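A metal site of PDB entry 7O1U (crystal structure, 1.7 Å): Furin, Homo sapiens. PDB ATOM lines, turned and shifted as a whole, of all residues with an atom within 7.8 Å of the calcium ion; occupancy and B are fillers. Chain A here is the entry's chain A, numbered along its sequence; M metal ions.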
ATOM      1  N   PRO A   6     -17.648  21.064  27.207  1.00  0.00           N
ATOM      2  CA  PRO A   6     -16.482  20.674  26.405  1.00  0.00           C
ATOM      3  C   PRO A   6     -15.542  19.736  27.140  1.00  0.00           C
ATOM      4  O   PRO A   6     -15.378  19.791  28.355  1.00  0.00           O
ATOM      5  CB  PRO A   6     -15.797  22.016  26.111  1.00  0.00           C
ATOM      6  CG  PRO A   6     -16.909  23.006  26.136  1.00  0.00           C
ATOM      7  CD  PRO A   6     -17.838  22.529  27.233  1.00  0.00           C
ATOM      8  N   THR A   7     -14.896  18.875  26.339  1.00  0.00           N
ATOM      9  CA  THR A   7     -13.933  17.898  26.815  1.00  0.00           C
ATOM     10  C   THR A   7     -12.498  18.315  26.534  1.00  0.00           C
ATOM     11  O   THR A   7     -11.574  17.555  26.851  1.00  0.00           O
ATOM     12  CB  THR A   7     -14.215  16.548  26.142  1.00  0.00           C
ATOM     13  OG1 THR A   7     -14.081  16.690  24.727  1.00  0.00           O
ATOM     14  CG2 THR A   7     -15.632  16.058  26.465  1.00  0.00           C
ATOM     15  N   ASP A   8     -12.290  19.488  25.953  1.00  0.00           N
ATOM     16  CA  ASP A   8     -10.959  19.937  25.564  1.00  0.00           C
ATOM     17  C   ASP A   8     -10.012  19.921  26.773  1.00  0.00           C
ATOM     18  O   ASP A   8     -10.425  20.213  27.895  1.00  0.00           O
ATOM     19  CB  ASP A   8     -11.032  21.335  24.961  1.00  0.00           C
ATOM     20  CG  ASP A   8     -11.997  21.414  23.795  1.00  0.00           C
ATOM     21  OD1 ASP A   8     -13.212  21.213  24.015  1.00  0.00           O
ATOM     22  OD2 ASP A   8     -11.548  21.677  22.661  1.00  0.00           O
ATOM     23  N   PRO A   9      -8.738  19.589  26.551  1.00  0.00           N
ATOM     24  CA  PRO A   9      -7.833  19.350  27.688  1.00  0.00           C
ATOM     25  C   PRO A   9      -7.618  20.542  28.595  1.00  0.00           C
ATOM     26  O   PRO A   9      -7.401  20.361  29.792  1.00  0.00           O
ATOM     27  CB  PRO A   9      -6.517  18.914  27.017  1.00  0.00           C
ATOM     28  CG  PRO A   9      -6.605  19.427  25.611  1.00  0.00           C
ATOM     29  CD  PRO A   9      -8.069  19.373  25.252  1.00  0.00           C
ATOM     30  N   LYS A  10      -7.663  21.763  28.062  1.00  0.00           N
ATOM     31  CA  LYS A  10      -7.459  22.956  28.877  1.00  0.00           C
ATOM     32  C   LYS A  10      -8.762  23.647  29.254  1.00  0.00           C
ATOM     33  O   LYS A  10      -8.722  24.711  29.892  1.00  0.00           O
ATOM     34  CB  LYS A  10      -6.537  23.952  28.138  1.00  0.00           C
ATOM     35  CG  LYS A  10      -5.102  23.429  27.928  1.00  0.00           C
ATOM     36  CD  LYS A  10      -4.382  23.244  29.274  1.00  0.00           C
ATOM     37  CE  LYS A  10      -2.957  22.727  29.116  1.00  0.00           C
ATOM     38  N   PHE A  11      -9.913  23.077  28.906  1.00  0.00           N
ATOM     39  CA  PHE A  11     -11.163  23.696  29.317  1.00  0.00           C
ATOM     40  C   PHE A  11     -11.238  23.841  30.840  1.00  0.00           C
ATOM     41  O   PHE A  11     -11.691  24.903  31.307  1.00  0.00           O
ATOM     42  CB  PHE A  11     -12.373  22.914  28.804  1.00  0.00           C
ATOM     43  CG  PHE A  11     -13.693  23.481  29.273  1.00  0.00           C
ATOM     44  CD1 PHE A  11     -14.101  24.743  28.866  1.00  0.00           C
ATOM     45  CD2 PHE A  11     -14.493  22.769  30.137  1.00  0.00           C
ATOM     46  CE1 PHE A  11     -15.307  25.283  29.303  1.00  0.00           C
ATOM     47  CE2 PHE A  11     -15.695  23.287  30.577  1.00  0.00           C
ATOM     48  CZ  PHE A  11     -16.105  24.547  30.161  1.00  0.00           C
ATOM     49  N   GLN A  14      -9.923  27.092  31.980  1.00  0.00           N
ATOM     50  CA  GLN A  14     -10.629  28.303  31.546  1.00  0.00           C
ATOM     51  C   GLN A  14     -11.644  28.677  32.620  1.00  0.00           C
ATOM     52  O   GLN A  14     -12.862  28.589  32.464  1.00  0.00           O
ATOM     53  CB  GLN A  14     -11.259  28.078  30.177  1.00  0.00           C
ATOM     54  CG  GLN A  14     -10.207  27.833  29.111  1.00  0.00           C
ATOM     55  CD  GLN A  14     -10.765  27.687  27.710  1.00  0.00           C
ATOM     56  OE1 GLN A  14     -11.500  26.745  27.414  1.00  0.00           O
ATOM     57  NE2 GLN A  14     -10.411  28.625  26.840  1.00  0.00           N
ATOM     58  N   PRO A  54      -4.501  24.492  14.732  1.00  0.00           N
ATOM     59  CA  PRO A  54      -5.411  23.328  14.916  1.00  0.00           C
ATOM     60  C   PRO A  54      -6.692  23.655  15.673  1.00  0.00           C
ATOM     61  O   PRO A  54      -7.673  22.894  15.533  1.00  0.00           O
ATOM     62  CB  PRO A  54      -4.556  22.314  15.695  1.00  0.00           C
ATOM     63  CG  PRO A  54      -3.147  22.712  15.445  1.00  0.00           C
ATOM     64  CD  PRO A  54      -3.148  24.202  15.256  1.00  0.00           C
ATOM     65  N   ASP A  55      -6.738  24.709  16.478  1.00  0.00           N
ATOM     66  CA  ASP A  55      -7.949  25.051  17.206  1.00  0.00           C
ATOM     67  C   ASP A  55      -8.705  26.219  16.583  1.00  0.00           C
ATOM     68  O   ASP A  55      -9.746  26.623  17.125  1.00  0.00           O
ATOM     69  CB  ASP A  55      -7.634  25.377  18.668  1.00  0.00           C
ATOM     70  CG  ASP A  55      -8.565  24.657  19.657  1.00  0.00           C
ATOM     71  OD1 ASP A  55      -9.162  23.617  19.287  1.00  0.00           O
ATOM     72  OD2 ASP A  55      -8.711  25.141  20.795  1.00  0.00           O
ATOM     73  N   LEU A  56      -8.232  26.763  15.451  1.00  0.00           N
ATOM     74  CA  LEU A  56      -8.943  27.799  14.718  1.00  0.00           C
ATOM     75  C   LEU A  56      -9.400  27.379  13.317  1.00  0.00           C
ATOM     76  O   LEU A  56     -10.409  27.894  12.838  1.00  0.00           O
ATOM     77  CB  LEU A  56      -8.085  29.062  14.558  1.00  0.00           C
ATOM     78  CG  LEU A  56      -7.618  29.702  15.871  1.00  0.00           C
ATOM     79  CD1 LEU A  56      -6.692  30.862  15.580  1.00  0.00           C
ATOM     80  CD2 LEU A  56      -8.809  30.137  16.701  1.00  0.00           C
ATOM     81  N   ALA A  96     -13.481  31.985  19.501  1.00  0.00           N
ATOM     82  CA  ALA A  96     -14.010  30.921  18.672  1.00  0.00           C
ATOM     83  C   ALA A  96     -13.064  29.739  18.482  1.00  0.00           C
ATOM     84  O   ALA A  96     -13.102  29.080  17.441  1.00  0.00           O
ATOM     85  CB  ALA A  96     -14.393  31.475  17.292  1.00  0.00           C
ATOM     86  N   ALA A  97     -12.227  29.445  19.468  1.00  0.00           N
ATOM     87  CA  ALA A  97     -11.489  28.195  19.422  1.00  0.00           C
ATOM     88  C   ALA A  97     -12.463  27.027  19.360  1.00  0.00           C
ATOM     89  O   ALA A  97     -13.493  27.003  20.047  1.00  0.00           O
ATOM     90  CB  ALA A  97     -10.575  28.054  20.642  1.00  0.00           C
ATOM     91  N   VAL A  98     -12.123  26.033  18.519  1.00  0.00           N
ATOM     92  CA  VAL A  98     -12.965  24.873  18.301  1.00  0.00           C
ATOM     93  C   VAL A  98     -13.115  24.075  19.578  1.00  0.00           C
ATOM     94  O   VAL A  98     -12.179  23.952  20.372  1.00  0.00           O
ATOM     95  CB  VAL A  98     -12.359  24.010  17.175  1.00  0.00           C
ATOM     96  CG1 VAL A  98     -13.118  22.689  17.033  1.00  0.00           C
ATOM     97  CG2 VAL A  98     -12.354  24.772  15.855  1.00  0.00           C
ATOM     98  N   ALA A  99     -14.302  23.493  19.773  1.00  0.00           N
ATOM     99  CA  ALA A  99     -14.604  22.715  20.965  1.00  0.00           C
ATOM    100  C   ALA A  99     -14.588  21.225  20.670  1.00  0.00           C
ATOM    101  O   ALA A  99     -14.841  20.791  19.539  1.00  0.00           O
ATOM    102  CB  ALA A  99     -15.967  23.114  21.539  1.00  0.00           C
ATOM    103  N   ASN A 100     -14.288  20.437  21.707  1.00  0.00           N
ATOM    104  CA  ASN A 100     -14.411  18.974  21.689  1.00  0.00           C
ATOM    105  C   ASN A 100     -13.526  18.326  20.625  1.00  0.00           C
ATOM    106  O   ASN A 100     -13.878  17.315  20.027  1.00  0.00           O
ATOM    107  CB  ASN A 100     -15.875  18.573  21.504  1.00  0.00           C
ATOM    108  CG  ASN A 100     -16.745  19.035  22.653  1.00  0.00           C
ATOM    109  OD1 ASN A 100     -16.474  18.729  23.811  1.00  0.00           O
ATOM    110  ND2 ASN A 100     -17.790  19.803  22.341  1.00  0.00           N
ATOM    111  N   ASN A 101     -12.327  18.892  20.431  1.00  0.00           N
ATOM    112  CA  ASN A 101     -11.391  18.398  19.430  1.00  0.00           C
ATOM    113  C   ASN A 101     -10.040  18.007  20.026  1.00  0.00           C
ATOM    114  O   ASN A 101      -9.073  17.856  19.274  1.00  0.00           O
ATOM    115  CB  ASN A 101     -11.207  19.451  18.335  1.00  0.00           C
ATOM    116  CG  ASN A 101     -10.472  20.675  18.815  1.00  0.00           C
ATOM    117  OD1 ASN A 101     -10.448  20.975  20.004  1.00  0.00           O
ATOM    118  ND2 ASN A 101      -9.838  21.385  17.885  1.00  0.00           N
ATOM    119  N   GLY A 102      -9.945  17.861  21.349  1.00  0.00           N
ATOM    120  CA  GLY A 102      -8.717  17.416  21.963  1.00  0.00           C
ATOM    121  C   GLY A 102      -7.565  18.403  21.926  1.00  0.00           C
ATOM    122  O   GLY A 102      -6.427  18.006  22.186  1.00  0.00           O
ATOM    123  N   VAL A 103      -7.831  19.676  21.642  1.00  0.00           N
ATOM    124  CA  VAL A 103      -6.810  20.699  21.471  1.00  0.00           C
ATOM    125  C   VAL A 103      -7.145  21.898  22.354  1.00  0.00           C
ATOM    126  O   VAL A 103      -8.261  22.418  22.295  1.00  0.00           O
ATOM    127  CB  VAL A 103      -6.682  21.135  19.999  1.00  0.00           C
ATOM    128  CG1 VAL A 103      -5.680  22.270  19.862  1.00  0.00           C
ATOM    129  CG2 VAL A 103      -6.304  19.942  19.104  1.00  0.00           C
ATOM    130  N   CYS A 104      -6.181  22.313  23.182  1.00  0.00           N
ATOM    131  CA  CYS A 104      -6.232  23.550  23.994  1.00  0.00           C
ATOM    132  C   CYS A 104      -7.586  23.644  24.678  1.00  0.00           C
ATOM    133  O   CYS A 104      -8.008  22.661  25.311  1.00  0.00           O
ATOM    134  CB  CYS A 104      -5.848  24.723  23.081  1.00  0.00           C
ATOM    135  SG  CYS A 104      -5.341  26.260  23.927  1.00  0.00           S
ATOM    136  N   GLY A 105      -8.274  24.791  24.617  1.00  0.00           N
ATOM    137  CA  GLY A 105      -9.569  24.929  25.269  1.00  0.00           C
ATOM    138  C   GLY A 105     -10.654  25.222  24.245  1.00  0.00           C
ATOM    139  O   GLY A 105     -10.623  24.653  23.150  1.00  0.00           O
ATOM    140  N   VAL A 106     -11.591  26.114  24.574  1.00  0.00           N
ATOM    141  CA  VAL A 106     -12.676  26.447  23.667  1.00  0.00           C
ATOM    142  C   VAL A 106     -12.850  27.959  23.618  1.00  0.00           C
ATOM    143  O   VAL A 106     -12.500  28.689  24.554  1.00  0.00           O
ATOM    144  CB  VAL A 106     -14.017  25.791  24.068  1.00  0.00           C
ATOM    145  CG1 VAL A 106     -13.834  24.288  24.229  1.00  0.00           C
ATOM    146  CG2 VAL A 106     -14.573  26.430  25.331  1.00  0.00           C
ATOM    147  N   GLY A 107     -13.434  28.417  22.521  1.00  0.00           N
ATOM    148  CA  GLY A 107     -13.919  29.768  22.469  1.00  0.00           C
ATOM    149  C   GLY A 107     -15.228  29.961  23.228  1.00  0.00           C
ATOM    150  O   GLY A 107     -15.972  29.013  23.489  1.00  0.00           O
ATOM    151  N   TYR A 110     -17.900  28.927  20.391  1.00  0.00           N
ATOM    152  CA  TYR A 110     -17.027  27.954  19.760  1.00  0.00           C
ATOM    153  C   TYR A 110     -17.583  27.373  18.465  1.00  0.00           C
ATOM    154  O   TYR A 110     -16.889  26.577  17.818  1.00  0.00           O
ATOM    155  CB  TYR A 110     -16.680  26.835  20.747  1.00  0.00           C
ATOM    156  CG  TYR A 110     -17.813  26.080  21.402  1.00  0.00           C
ATOM    157  CD1 TYR A 110     -18.644  25.229  20.682  1.00  0.00           C
ATOM    158  CD2 TYR A 110     -18.020  26.171  22.778  1.00  0.00           C
ATOM    159  CE1 TYR A 110     -19.660  24.511  21.304  1.00  0.00           C
ATOM    160  CE2 TYR A 110     -19.032  25.468  23.406  1.00  0.00           C
ATOM    161  CZ  TYR A 110     -19.843  24.633  22.668  1.00  0.00           C
ATOM    162  OH  TYR A 110     -20.845  23.937  23.302  1.00  0.00           O
ATOM    163  N   THR A 247      -5.490  29.934  22.172  1.00  0.00           N
ATOM    164  CA  THR A 247      -4.595  29.556  21.084  1.00  0.00           C
ATOM    165  C   THR A 247      -3.416  30.512  20.995  1.00  0.00           C
ATOM    166  O   THR A 247      -3.562  31.725  21.186  1.00  0.00           O
ATOM    167  CB  THR A 247      -5.372  29.573  19.774  1.00  0.00           C
ATOM    168  OG1 THR A 247      -6.101  30.813  19.684  1.00  0.00           O
ATOM    169  CG2 THR A 247      -6.369  28.450  19.740  1.00  0.00           C
HETATM  170 CA    CA M   1     -10.241  23.126  21.350  1.00  0.00          CA
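OD1 of Asp 8 sits at hydrogen-bond distance from N of Asn 100 (2.7 Å).
Of the 24 residues printed, 6 come within 4 Å of the calcium ion.
The nearest printed residue that does not touch the calcium ion is Cys 104 (4.3 Å).
The calcium ion is bound by the backbone carbonyl oxygen (O) of Val 103 (2.3 Å), the backbone carbonyl oxygen (O) of Val 98 (2.3 Å), the side-chain carboxylate (OD2) of Asp 8 (2.4 Å), the side-chain carboxylate (OD1) of Asp 55 (2.4 Å), the backbone carbonyl oxygen (O) of Gly 105 (2.4 Å), the side-chain amide oxygen (OD1) of Asn 101 (2.5 Å) and the side-chain carboxylate (OD2) of Asp 55 (2.6 Å).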
